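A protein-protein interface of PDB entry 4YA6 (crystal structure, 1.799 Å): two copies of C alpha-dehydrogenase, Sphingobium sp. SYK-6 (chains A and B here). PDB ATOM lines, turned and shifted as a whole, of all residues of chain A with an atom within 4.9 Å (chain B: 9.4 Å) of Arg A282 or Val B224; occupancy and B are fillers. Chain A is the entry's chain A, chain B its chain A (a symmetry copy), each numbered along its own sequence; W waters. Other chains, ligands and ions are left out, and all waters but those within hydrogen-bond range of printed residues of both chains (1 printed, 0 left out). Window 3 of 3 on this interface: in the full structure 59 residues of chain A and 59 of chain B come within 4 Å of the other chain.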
ATOM      1  N   ASP A 278     -14.939 -15.018  -5.917  1.00  0.00           N
ATOM      2  CA  ASP A 278     -14.824 -15.434  -4.516  1.00  0.00           C
ATOM      3  C   ASP A 278     -15.946 -14.854  -3.662  1.00  0.00           C
ATOM      4  O   ASP A 278     -16.381 -15.478  -2.697  1.00  0.00           O
ATOM      5  CB  ASP A 278     -13.470 -15.023  -3.928  1.00  0.00           C
ATOM      6  CG  ASP A 278     -12.327 -15.901  -4.414  1.00  0.00           C
ATOM      7  OD1 ASP A 278     -12.582 -17.053  -4.819  1.00  0.00           O
ATOM      8  OD2 ASP A 278     -11.166 -15.441  -4.375  1.00  0.00           O
ATOM      9  N   TYR A 279     -16.416 -13.665  -4.021  1.00  0.00           N
ATOM     10  CA  TYR A 279     -17.514 -13.040  -3.295  1.00  0.00           C
ATOM     11  C   TYR A 279     -18.808 -13.821  -3.497  1.00  0.00           C
ATOM     12  O   TYR A 279     -19.520 -14.111  -2.538  1.00  0.00           O
ATOM     13  CB  TYR A 279     -17.699 -11.589  -3.737  1.00  0.00           C
ATOM     14  CG  TYR A 279     -19.014 -10.990  -3.293  1.00  0.00           C
ATOM     15  CD1 TYR A 279     -19.313 -10.842  -1.946  1.00  0.00           C
ATOM     16  CD2 TYR A 279     -19.954 -10.571  -4.222  1.00  0.00           C
ATOM     17  CE1 TYR A 279     -20.516 -10.299  -1.537  1.00  0.00           C
ATOM     18  CE2 TYR A 279     -21.158 -10.024  -3.823  1.00  0.00           C
ATOM     19  CZ  TYR A 279     -21.434  -9.889  -2.480  1.00  0.00           C
ATOM     20  OH  TYR A 279     -22.631  -9.345  -2.075  1.00  0.00           O
ATOM     21  N   ALA A 280     -19.107 -14.165  -4.746  1.00  0.00           N
ATOM     22  CA  ALA A 280     -20.288 -14.962  -5.054  1.00  0.00           C
ATOM     23  C   ALA A 280     -20.207 -16.314  -4.353  1.00  0.00           C
ATOM     24  O   ALA A 280     -21.224 -16.882  -3.959  1.00  0.00           O
ATOM     25  CB  ALA A 280     -20.433 -15.146  -6.554  1.00  0.00           C
ATOM     26  N   ARG A 281     -18.986 -16.821  -4.200  1.00  0.00           N
ATOM     27  CA  ARG A 281     -18.757 -18.076  -3.496  1.00  0.00           C
ATOM     28  C   ARG A 281     -19.079 -17.939  -2.010  1.00  0.00           C
ATOM     29  O   ARG A 281     -19.710 -18.819  -1.424  1.00  0.00           O
ATOM     30  CB  ARG A 281     -17.310 -18.540  -3.691  1.00  0.00           C
ATOM     31  CG  ARG A 281     -17.091 -19.308  -4.987  1.00  0.00           C
ATOM     32  CD  ARG A 281     -15.693 -19.113  -5.560  1.00  0.00           C
ATOM     33  NE  ARG A 281     -14.654 -19.756  -4.761  1.00  0.00           N
ATOM     34  CZ  ARG A 281     -13.399 -19.927  -5.167  1.00  0.00           C
ATOM     35  NH1 ARG A 281     -13.021 -19.506  -6.367  1.00  0.00           N
ATOM     36  NH2 ARG A 281     -12.518 -20.523  -4.375  1.00  0.00           N
ATOM     37  N   ARG A 282     -18.653 -16.833  -1.405  1.00  0.00           N
ATOM     38  CA  ARG A 282     -18.949 -16.573   0.001  1.00  0.00           C
ATOM     39  C   ARG A 282     -20.447 -16.370   0.207  1.00  0.00           C
ATOM     40  O   ARG A 282     -21.000 -16.763   1.235  1.00  0.00           O
ATOM     41  CB  ARG A 282     -18.173 -15.351   0.506  1.00  0.00           C
ATOM     42  CG  ARG A 282     -16.673 -15.581   0.633  1.00  0.00           C
ATOM     43  CD  ARG A 282     -15.992 -14.499   1.461  1.00  0.00           C
ATOM     44  NE  ARG A 282     -16.174 -13.163   0.900  1.00  0.00           N
ATOM     45  CZ  ARG A 282     -15.431 -12.641  -0.073  1.00  0.00           C
ATOM     46  NH1 ARG A 282     -14.447 -13.344  -0.619  1.00  0.00           N
ATOM     47  NH2 ARG A 282     -15.679 -11.414  -0.507  1.00  0.00           N
ATOM     48  N   MET A 283     -21.103 -15.761  -0.777  1.00  0.00           N
ATOM     49  CA  MET A 283     -22.542 -15.535  -0.710  1.00  0.00           C
ATOM     50  C   MET A 283     -23.304 -16.844  -0.880  1.00  0.00           C
ATOM     51  O   MET A 283     -24.370 -17.028  -0.292  1.00  0.00           O
ATOM     52  CB  MET A 283     -22.978 -14.525  -1.775  1.00  0.00           C
ATOM     53  CG  MET A 283     -22.492 -13.098  -1.528  1.00  0.00           C
ATOM     54  SD  MET A 283     -22.945 -12.438   0.091  1.00  0.00           S
ATOM     55  CE  MET A 283     -21.521 -12.907   1.076  1.00  0.00           C
ATOM     56  N   LYS A 284     -22.755 -17.750  -1.683  1.00  0.00           N
ATOM     57  CA  LYS A 284     -23.357 -19.064  -1.867  1.00  0.00           C
ATOM     58  C   LYS A 284     -23.358 -19.825  -0.544  1.00  0.00           C
ATOM     59  O   LYS A 284     -24.324 -20.509  -0.209  1.00  0.00           O
ATOM     60  CB  LYS A 284     -22.606 -19.860  -2.938  1.00  0.00           C
ATOM     61  CG  LYS A 284     -23.246 -21.201  -3.276  1.00  0.00           C
ATOM     62  CD  LYS A 284     -22.488 -21.935  -4.377  1.00  0.00           C
ATOM     63  CE  LYS A 284     -21.145 -22.468  -3.895  1.00  0.00           C
ATOM     64  NZ  LYS A 284     -21.289 -23.470  -2.801  1.00  0.00           N
ATOM     65  N   ILE A 285     -22.271 -19.689   0.207  1.00  0.00           N
ATOM     66  CA  ILE A 285     -22.129 -20.372   1.487  1.00  0.00           C
ATOM     67  C   ILE A 285     -23.086 -19.791   2.529  1.00  0.00           C
ATOM     68  O   ILE A 285     -23.705 -20.536   3.289  1.00  0.00           O
ATOM     69  CB  ILE A 285     -20.672 -20.288   2.002  1.00  0.00           C
ATOM     70  CG1 ILE A 285     -19.753 -21.094   1.080  1.00  0.00           C
ATOM     71  CG2 ILE A 285     -20.564 -20.811   3.436  1.00  0.00           C
ATOM     72  CD1 ILE A 285     -18.273 -20.951   1.381  1.00  0.00           C
ATOM     73  N   ARG A 286     -23.202 -18.466   2.563  1.00  0.00           N
ATOM     74  CA  ARG A 286     -24.087 -17.807   3.518  1.00  0.00           C
ATOM     75  C   ARG A 286     -25.546 -18.172   3.253  1.00  0.00           C
ATOM     76  O   ARG A 286     -26.299 -18.460   4.182  1.00  0.00           O
ATOM     77  CB  ARG A 286     -23.908 -16.289   3.464  1.00  0.00           C
ATOM     78  CG  ARG A 286     -24.823 -15.531   4.415  1.00  0.00           C
ATOM     79  CD  ARG A 286     -24.363 -14.096   4.618  1.00  0.00           C
ATOM     80  NE  ARG A 286     -25.169 -13.402   5.619  1.00  0.00           N
ATOM     81  CZ  ARG A 286     -24.963 -13.466   6.933  1.00  0.00           C
ATOM     82  NH1 ARG A 286     -23.971 -14.198   7.423  1.00  0.00           N
ATOM     83  NH2 ARG A 286     -25.753 -12.796   7.760  1.00  0.00           N
ATOM     84  N   PRO B 187      -7.559  -6.212   5.695  1.00  0.00           N
ATOM     85  CA  PRO B 187      -7.922  -7.630   5.605  1.00  0.00           C
ATOM     86  C   PRO B 187      -8.955  -8.045   6.648  1.00  0.00           C
ATOM     87  O   PRO B 187      -9.818  -8.876   6.362  1.00  0.00           O
ATOM     88  CB  PRO B 187      -6.593  -8.359   5.858  1.00  0.00           C
ATOM     89  CG  PRO B 187      -5.525  -7.314   5.786  1.00  0.00           C
ATOM     90  CD  PRO B 187      -6.178  -6.034   6.174  1.00  0.00           C
ATOM     91  N   VAL B 217     -23.612 -10.073  13.232  1.00  0.00           N
ATOM     92  CA  VAL B 217     -23.640 -10.274  11.791  1.00  0.00           C
ATOM     93  C   VAL B 217     -22.257 -10.060  11.184  1.00  0.00           C
ATOM     94  O   VAL B 217     -21.831 -10.826  10.322  1.00  0.00           O
ATOM     95  CB  VAL B 217     -24.665  -9.316  11.131  1.00  0.00           C
ATOM     96  CG1 VAL B 217     -24.455  -9.211   9.620  1.00  0.00           C
ATOM     97  CG2 VAL B 217     -26.083  -9.773  11.446  1.00  0.00           C
ATOM     98  N   PHE B 218     -21.564  -9.018  11.632  1.00  0.00           N
ATOM     99  CA  PHE B 218     -20.225  -8.724  11.133  1.00  0.00           C
ATOM    100  C   PHE B 218     -19.279  -9.882  11.421  1.00  0.00           C
ATOM    101  O   PHE B 218     -18.475 -10.267  10.571  1.00  0.00           O
ATOM    102  CB  PHE B 218     -19.676  -7.442  11.757  1.00  0.00           C
ATOM    103  CG  PHE B 218     -18.296  -7.084  11.281  1.00  0.00           C
ATOM    104  CD1 PHE B 218     -18.119  -6.363  10.113  1.00  0.00           C
ATOM    105  CD2 PHE B 218     -17.177  -7.477  11.996  1.00  0.00           C
ATOM    106  CE1 PHE B 218     -16.851  -6.036   9.668  1.00  0.00           C
ATOM    107  CE2 PHE B 218     -15.906  -7.154  11.557  1.00  0.00           C
ATOM    108  CZ  PHE B 218     -15.743  -6.432  10.391  1.00  0.00           C
ATOM    109  N   ALA B 219     -19.380 -10.430  12.627  1.00  0.00           N
ATOM    110  CA  ALA B 219     -18.560 -11.564  13.031  1.00  0.00           C
ATOM    111  C   ALA B 219     -18.805 -12.759  12.118  1.00  0.00           C
ATOM    112  O   ALA B 219     -17.864 -13.408  11.661  1.00  0.00           O
ATOM    113  CB  ALA B 219     -18.846 -11.935  14.476  1.00  0.00           C
ATOM    114  N   GLY B 220     -20.077 -13.041  11.854  1.00  0.00           N
ATOM    115  CA  GLY B 220     -20.456 -14.157  11.009  1.00  0.00           C
ATOM    116  C   GLY B 220     -19.986 -13.984   9.578  1.00  0.00           C
ATOM    117  O   GLY B 220     -19.583 -14.949   8.929  1.00  0.00           O
ATOM    118  N   LEU B 221     -20.037 -12.752   9.083  1.00  0.00           N
ATOM    119  CA  LEU B 221     -19.578 -12.457   7.732  1.00  0.00           C
ATOM    120  C   LEU B 221     -18.060 -12.555   7.646  1.00  0.00           C
ATOM    121  O   LEU B 221     -17.519 -13.067   6.665  1.00  0.00           O
ATOM    122  CB  LEU B 221     -20.036 -11.062   7.293  1.00  0.00           C
ATOM    123  CG  LEU B 221     -21.531 -10.858   7.033  1.00  0.00           C
ATOM    124  CD1 LEU B 221     -21.794  -9.420   6.615  1.00  0.00           C
ATOM    125  CD2 LEU B 221     -22.054 -11.826   5.978  1.00  0.00           C
ATOM    126  N   LYS B 222     -17.375 -12.067   8.675  1.00  0.00           N
ATOM    127  CA  LYS B 222     -15.917 -12.091   8.691  1.00  0.00           C
ATOM    128  C   LYS B 222     -15.396 -13.519   8.809  1.00  0.00           C
ATOM    129  O   LYS B 222     -14.343 -13.845   8.266  1.00  0.00           O
ATOM    130  CB  LYS B 222     -15.368 -11.237   9.839  1.00  0.00           C
ATOM    131  CG  LYS B 222     -13.856 -11.062   9.789  1.00  0.00           C
ATOM    132  CD  LYS B 222     -13.352 -10.031  10.788  1.00  0.00           C
ATOM    133  CE  LYS B 222     -13.361 -10.565  12.210  1.00  0.00           C
ATOM    134  NZ  LYS B 222     -12.579  -9.694  13.132  1.00  0.00           N
ATOM    135  N   ARG B 223     -16.134 -14.369   9.515  1.00  0.00           N
ATOM    136  CA  ARG B 223     -15.711 -15.751   9.719  1.00  0.00           C
ATOM    137  C   ARG B 223     -15.675 -16.527   8.403  1.00  0.00           C
ATOM    138  O   ARG B 223     -14.790 -17.354   8.187  1.00  0.00           O
ATOM    139  CB  ARG B 223     -16.633 -16.456  10.716  1.00  0.00           C
ATOM    140  CG  ARG B 223     -16.290 -17.920  10.923  1.00  0.00           C
ATOM    141  CD  ARG B 223     -16.747 -18.424  12.279  1.00  0.00           C
ATOM    142  NE  ARG B 223     -16.317 -19.801  12.516  1.00  0.00           N
ATOM    143  CZ  ARG B 223     -15.112 -20.150  12.954  1.00  0.00           C
ATOM    144  NH1 ARG B 223     -14.194 -19.226  13.209  1.00  0.00           N
ATOM    145  NH2 ARG B 223     -14.818 -21.432  13.136  1.00  0.00           N
ATOM    146  N   VAL B 224     -16.637 -16.258   7.527  1.00  0.00           N
ATOM    147  CA  VAL B 224     -16.665 -16.895   6.215  1.00  0.00           C
ATOM    148  C   VAL B 224     -15.501 -16.375   5.370  1.00  0.00           C
ATOM    149  O   VAL B 224     -14.916 -17.118   4.582  1.00  0.00           O
ATOM    150  CB  VAL B 224     -18.017 -16.652   5.503  1.00  0.00           C
ATOM    151  CG1 VAL B 224     -17.898 -16.825   3.988  1.00  0.00           C
ATOM    152  CG2 VAL B 224     -19.074 -17.595   6.062  1.00  0.00           C
ATOM    153  N   ILE B 225     -15.165 -15.101   5.544  1.00  0.00           N
ATOM    154  CA  ILE B 225     -14.006 -14.523   4.874  1.00  0.00           C
ATOM    155  C   ILE B 225     -12.731 -15.173   5.403  1.00  0.00           C
ATOM    156  O   ILE B 225     -11.820 -15.482   4.635  1.00  0.00           O
ATOM    157  CB  ILE B 225     -13.942 -12.992   5.073  1.00  0.00           C
ATOM    158  CG1 ILE B 225     -15.083 -12.315   4.310  1.00  0.00           C
ATOM    159  CG2 ILE B 225     -12.599 -12.435   4.599  1.00  0.00           C
ATOM    160  CD1 ILE B 225     -15.299 -10.864   4.680  1.00  0.00           C
ATOM    161  N   GLU B 226     -12.676 -15.374   6.716  1.00  0.00           N
ATOM    162  CA  GLU B 226     -11.543 -16.036   7.352  1.00  0.00           C
ATOM    163  C   GLU B 226     -11.334 -17.434   6.780  1.00  0.00           C
ATOM    164  O   GLU B 226     -10.203 -17.878   6.587  1.00  0.00           O
ATOM    165  CB  GLU B 226     -11.751 -16.124   8.867  1.00  0.00           C
ATOM    166  CG  GLU B 226     -11.615 -14.802   9.607  1.00  0.00           C
ATOM    167  CD  GLU B 226     -12.176 -14.860  11.017  1.00  0.00           C
ATOM    168  OE1 GLU B 226     -12.517 -15.969  11.481  1.00  0.00           O
ATOM    169  OE2 GLU B 226     -12.276 -13.797  11.663  1.00  0.00           O
ATOM    170  N   HIS B 227     -12.439 -18.121   6.503  1.00  0.00           N
ATOM    171  CA  HIS B 227     -12.392 -19.498   6.028  1.00  0.00           C
ATOM    172  C   HIS B 227     -11.829 -19.610   4.614  1.00  0.00           C
ATOM    173  O   HIS B 227     -11.169 -20.595   4.279  1.00  0.00           O
ATOM    174  CB  HIS B 227     -13.791 -20.115   6.076  1.00  0.00           C
ATOM    175  CG  HIS B 227     -14.263 -20.428   7.461  1.00  0.00           C
ATOM    176  ND1 HIS B 227     -13.399 -20.574   8.525  1.00  0.00           N
ATOM    177  CD2 HIS B 227     -15.507 -20.627   7.956  1.00  0.00           C
ATOM    178  CE1 HIS B 227     -14.091 -20.849   9.617  1.00  0.00           C
ATOM    179  NE2 HIS B 227     -15.372 -20.885   9.298  1.00  0.00           N
ATOM    180  N   GLY B 228     -12.091 -18.600   3.792  1.00  0.00           N
ATOM    181  CA  GLY B 228     -11.648 -18.605   2.408  1.00  0.00           C
ATOM    182  C   GLY B 228     -10.375 -17.813   2.188  1.00  0.00           C
ATOM    183  O   GLY B 228      -9.802 -17.841   1.100  1.00  0.00           O
ATOM    184  N   PHE B 229      -9.932 -17.110   3.224  1.00  0.00           N
ATOM    185  CA  PHE B 229      -8.759 -16.252   3.121  1.00  0.00           C
ATOM    186  C   PHE B 229      -7.505 -17.010   2.694  1.00  0.00           C
ATOM    187  O   PHE B 229      -7.240 -18.115   3.168  1.00  0.00           O
ATOM    188  CB  PHE B 229      -8.493 -15.554   4.453  1.00  0.00           C
ATOM    189  CG  PHE B 229      -7.200 -14.802   4.480  1.00  0.00           C
ATOM    190  CD1 PHE B 229      -7.083 -13.588   3.829  1.00  0.00           C
ATOM    191  CD2 PHE B 229      -6.097 -15.314   5.141  1.00  0.00           C
ATOM    192  CE1 PHE B 229      -5.895 -12.895   3.844  1.00  0.00           C
ATOM    193  CE2 PHE B 229      -4.905 -14.623   5.159  1.00  0.00           C
ATOM    194  CZ  PHE B 229      -4.806 -13.413   4.509  1.00  0.00           C
ATOM    195  N   ASP B 230      -6.744 -16.398   1.791  1.00  0.00           N
ATOM    196  CA  ASP B 230      -5.467 -16.938   1.343  1.00  0.00           C
ATOM    197  C   ASP B 230      -4.461 -15.798   1.172  1.00  0.00           C
ATOM    198  O   ASP B 230      -4.761 -14.816   0.491  1.00  0.00           O
ATOM    199  CB  ASP B 230      -5.634 -17.704   0.030  1.00  0.00           C
ATOM    200  CG  ASP B 230      -4.311 -18.115  -0.576  1.00  0.00           C
ATOM    201  OD1 ASP B 230      -3.676 -19.048  -0.042  1.00  0.00           O
ATOM    202  OD2 ASP B 230      -3.908 -17.509  -1.590  1.00  0.00           O
ATOM    203  N   ASP B 233      -3.683 -14.938  -2.535  1.00  0.00           N
ATOM    204  CA  ASP B 233      -4.821 -14.304  -3.190  1.00  0.00           C
ATOM    205  C   ASP B 233      -4.937 -12.845  -2.755  1.00  0.00           C
ATOM    206  O   ASP B 233      -5.156 -11.959  -3.580  1.00  0.00           O
ATOM    207  CB  ASP B 233      -6.118 -15.054  -2.880  1.00  0.00           C
ATOM    208  CG  ASP B 233      -6.138 -16.454  -3.466  1.00  0.00           C
ATOM    209  OD1 ASP B 233      -5.333 -16.731  -4.380  1.00  0.00           O
ATOM    210  OD2 ASP B 233      -6.964 -17.276  -3.019  1.00  0.00           O
ATOM    211  N   LEU B 234      -4.777 -12.600  -1.458  1.00  0.00           N
ATOM    212  CA  LEU B 234      -4.826 -11.239  -0.936  1.00  0.00           C
ATOM    213  C   LEU B 234      -3.625 -10.444  -1.444  1.00  0.00           C
ATOM    214  O   LEU B 234      -3.694  -9.224  -1.593  1.00  0.00           O
ATOM    215  CB  LEU B 234      -4.846 -11.242   0.596  1.00  0.00           C
ATOM    216  CG  LEU B 234      -5.856 -10.376   1.370  1.00  0.00           C
ATOM    217  CD1 LEU B 234      -5.154  -9.706   2.544  1.00  0.00           C
ATOM    218  CD2 LEU B 234      -6.575  -9.328   0.524  1.00  0.00           C
ATOM    219  N   VAL B 237      -4.527  -9.094  -4.778  1.00  0.00           N
ATOM    220  CA  VAL B 237      -5.401  -7.935  -4.613  1.00  0.00           C
ATOM    221  C   VAL B 237      -4.548  -6.686  -4.401  1.00  0.00           C
ATOM    222  O   VAL B 237      -4.809  -5.637  -4.990  1.00  0.00           O
ATOM    223  CB  VAL B 237      -6.374  -8.118  -3.424  1.00  0.00           C
ATOM    224  CG1 VAL B 237      -7.149  -6.830  -3.145  1.00  0.00           C
ATOM    225  CG2 VAL B 237      -7.332  -9.265  -3.697  1.00  0.00           C
ATOM    226  N   LEU B 250     -10.475  -2.668   0.277  1.00  0.00           N
ATOM    227  CA  LEU B 250     -11.337  -3.439   1.166  1.00  0.00           C
ATOM    228  C   LEU B 250     -12.212  -4.359   0.322  1.00  0.00           C
ATOM    229  O   LEU B 250     -13.385  -4.067   0.098  1.00  0.00           O
ATOM    230  CB  LEU B 250     -12.218  -2.524   2.019  1.00  0.00           C
ATOM    231  CG  LEU B 250     -11.530  -1.471   2.886  1.00  0.00           C
ATOM    232  CD1 LEU B 250     -11.260  -0.203   2.095  1.00  0.00           C
ATOM    233  CD2 LEU B 250     -12.387  -1.171   4.099  1.00  0.00           C
ATOM    234  N   PRO B 251     -11.642  -5.475  -0.153  1.00  0.00           N
ATOM    235  CA  PRO B 251     -12.316  -6.311  -1.151  1.00  0.00           C
ATOM    236  C   PRO B 251     -13.437  -7.175  -0.565  1.00  0.00           C
ATOM    237  O   PRO B 251     -13.457  -8.388  -0.773  1.00  0.00           O
ATOM    238  CB  PRO B 251     -11.170  -7.171  -1.691  1.00  0.00           C
ATOM    239  CG  PRO B 251     -10.266  -7.335  -0.527  1.00  0.00           C
ATOM    240  CD  PRO B 251     -10.331  -6.031   0.231  1.00  0.00           C
ATOM    241  N   TYR B 252     -14.372  -6.544   0.143  1.00  0.00           N
ATOM    242  CA  TYR B 252     -15.444  -7.267   0.821  1.00  0.00           C
ATOM    243  C   TYR B 252     -16.785  -6.548   0.703  1.00  0.00           C
ATOM    244  O   TYR B 252     -17.137  -5.738   1.561  1.00  0.00           O
ATOM    245  CB  TYR B 252     -15.082  -7.473   2.294  1.00  0.00           C
ATOM    246  CG  TYR B 252     -13.778  -8.212   2.479  1.00  0.00           C
ATOM    247  CD1 TYR B 252     -13.633  -9.518   2.025  1.00  0.00           C
ATOM    248  CD2 TYR B 252     -12.691  -7.609   3.098  1.00  0.00           C
ATOM    249  CE1 TYR B 252     -12.444 -10.201   2.183  1.00  0.00           C
ATOM    250  CE2 TYR B 252     -11.496  -8.289   3.263  1.00  0.00           C
ATOM    251  CZ  TYR B 252     -11.379  -9.585   2.803  1.00  0.00           C
ATOM    252  OH  TYR B 252     -10.194 -10.269   2.962  1.00  0.00           O
ATOM    253  N   PRO B 253     -17.539  -6.839  -0.371  1.00  0.00           N
ATOM    254  CA  PRO B 253     -18.864  -6.244  -0.579  1.00  0.00           C
ATOM    255  C   PRO B 253     -19.846  -6.534   0.556  1.00  0.00           C
ATOM    256  O   PRO B 253     -20.780  -5.759   0.755  1.00  0.00           O
ATOM    257  CB  PRO B 253     -19.343  -6.892  -1.884  1.00  0.00           C
ATOM    258  CG  PRO B 253     -18.103  -7.318  -2.582  1.00  0.00           C
ATOM    259  CD  PRO B 253     -17.130  -7.683  -1.509  1.00  0.00           C
ATOM    260  N   GLU B 254     -19.632  -7.627   1.287  1.00  0.00           N
ATOM    261  CA  GLU B 254     -20.535  -8.022   2.368  1.00  0.00           C
ATOM    262  C   GLU B 254     -20.681  -6.929   3.418  1.00  0.00           C
ATOM    263  O   GLU B 254     -21.760  -6.724   3.972  1.00  0.00           O
ATOM    264  CB  GLU B 254     -20.041  -9.297   3.055  1.00  0.00           C
ATOM    265  CG  GLU B 254     -19.701 -10.436   2.125  1.00  0.00           C
ATOM    266  CD  GLU B 254     -18.214 -10.554   1.870  1.00  0.00           C
ATOM    267  OE1 GLU B 254     -17.624  -9.600   1.324  1.00  0.00           O
ATOM    268  OE2 GLU B 254     -17.635 -11.601   2.228  1.00  0.00           O
ATOM    269  N   PHE B 255     -19.582  -6.234   3.690  1.00  0.00           N
ATOM    270  CA  PHE B 255     -19.533  -5.260   4.773  1.00  0.00           C
ATOM    271  C   PHE B 255     -20.201  -3.934   4.412  1.00  0.00           C
ATOM    272  O   PHE B 255     -20.261  -3.024   5.239  1.00  0.00           O
ATOM    273  CB  PHE B 255     -18.076  -5.004   5.174  1.00  0.00           C
ATOM    274  CG  PHE B 255     -17.383  -6.204   5.763  1.00  0.00           C
ATOM    275  CD1 PHE B 255     -18.078  -7.129   6.528  1.00  0.00           C
ATOM    276  CD2 PHE B 255     -16.028  -6.404   5.553  1.00  0.00           C
ATOM    277  CE1 PHE B 255     -17.435  -8.226   7.068  1.00  0.00           C
ATOM    278  CE2 PHE B 255     -15.381  -7.500   6.092  1.00  0.00           C
ATOM    279  CZ  PHE B 255     -16.086  -8.411   6.851  1.00  0.00           C
HETATM  280  O   HOH W   1     -13.672 -10.789  -2.393  1.00  0.00           O
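No position is printed for both chains.
Water W1 lies within hydrogen-bond range of NH2 of Arg A282 (2.8 Å) and O of Pro B251 (2.9 Å).
Of chain B, only Val B224 (3.8 Å), Ile B225 (3.7 Å), Pro B251 (3.8 Å), Tyr B252 (3.8 Å) and Glu B254 (2.5 Å) come within 4 Å of Arg A282.
Of chain A, only Arg A282 comes within 4 Å of Val B224.
Printed residues of chain B within 4 Å of Met A283: Glu B254.
No residue of chain B comes within 4 Å of Ile A285.
Of the printed residues of chain A, Pro B251 touches Arg A282 (3.8 Å).
Of the printed residues of chain B, Arg A286 touches Leu B221.
Of the printed residues of chain A, Leu B221 touches Arg A286 (3.4 Å).
Printed residues of chain B within 4 Å of Tyr A279: Pro B253 (3.6 Å) and Glu B254 (3.8 Å).
Printed residues of chain A within 4 Å of Tyr B252: Arg A282 (3.8 Å).
The nearest residue of chain B that does not touch Arg A282 is Pro B253 (4.1 Å).
The nearest residue of chain A that does not touch Val B224 is Ile A285 (4.4 Å).
The side-chain hydroxyl of Tyr A279 sits close to the side-chain sulfur of Met A283 (3.8 Å).
Hydrophobic or aromatic side chains of chain B that line the printed part of chain A: Leu B221, Val B224, Ile B225, Tyr B252 and Pro B253.
Of the 9 printed residues of chain A, 4 touch a printed residue of chain B.
Printed residues of chain A that touch a printed residue of chain B: Tyr A279, Arg A282, Met A283 and Arg A286.
Among the printed residues, 9 pairs touch across the chains.
Among the printed residues, pairs that only touch across the chains: Tyr A279 with Pro B253 (3.6 Å), Tyr A279 with Glu B254 (3.8 Å), Arg A282 with Val B224 (3.8 Å), Arg A282 with Ile B225 (3.7 Å), Arg A282 with Pro B251 (3.8 Å), Arg A282 with Tyr B252 (3.8 Å), Met A283 with Glu B254 (3.2 Å) and Arg A286 with Leu B221 (3.4 Å).
The guanidinium group (NE) of Arg A282 is in salt-bridge range of the side-chain carboxylate (OE2) of Glu B254 (2.5 Å).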
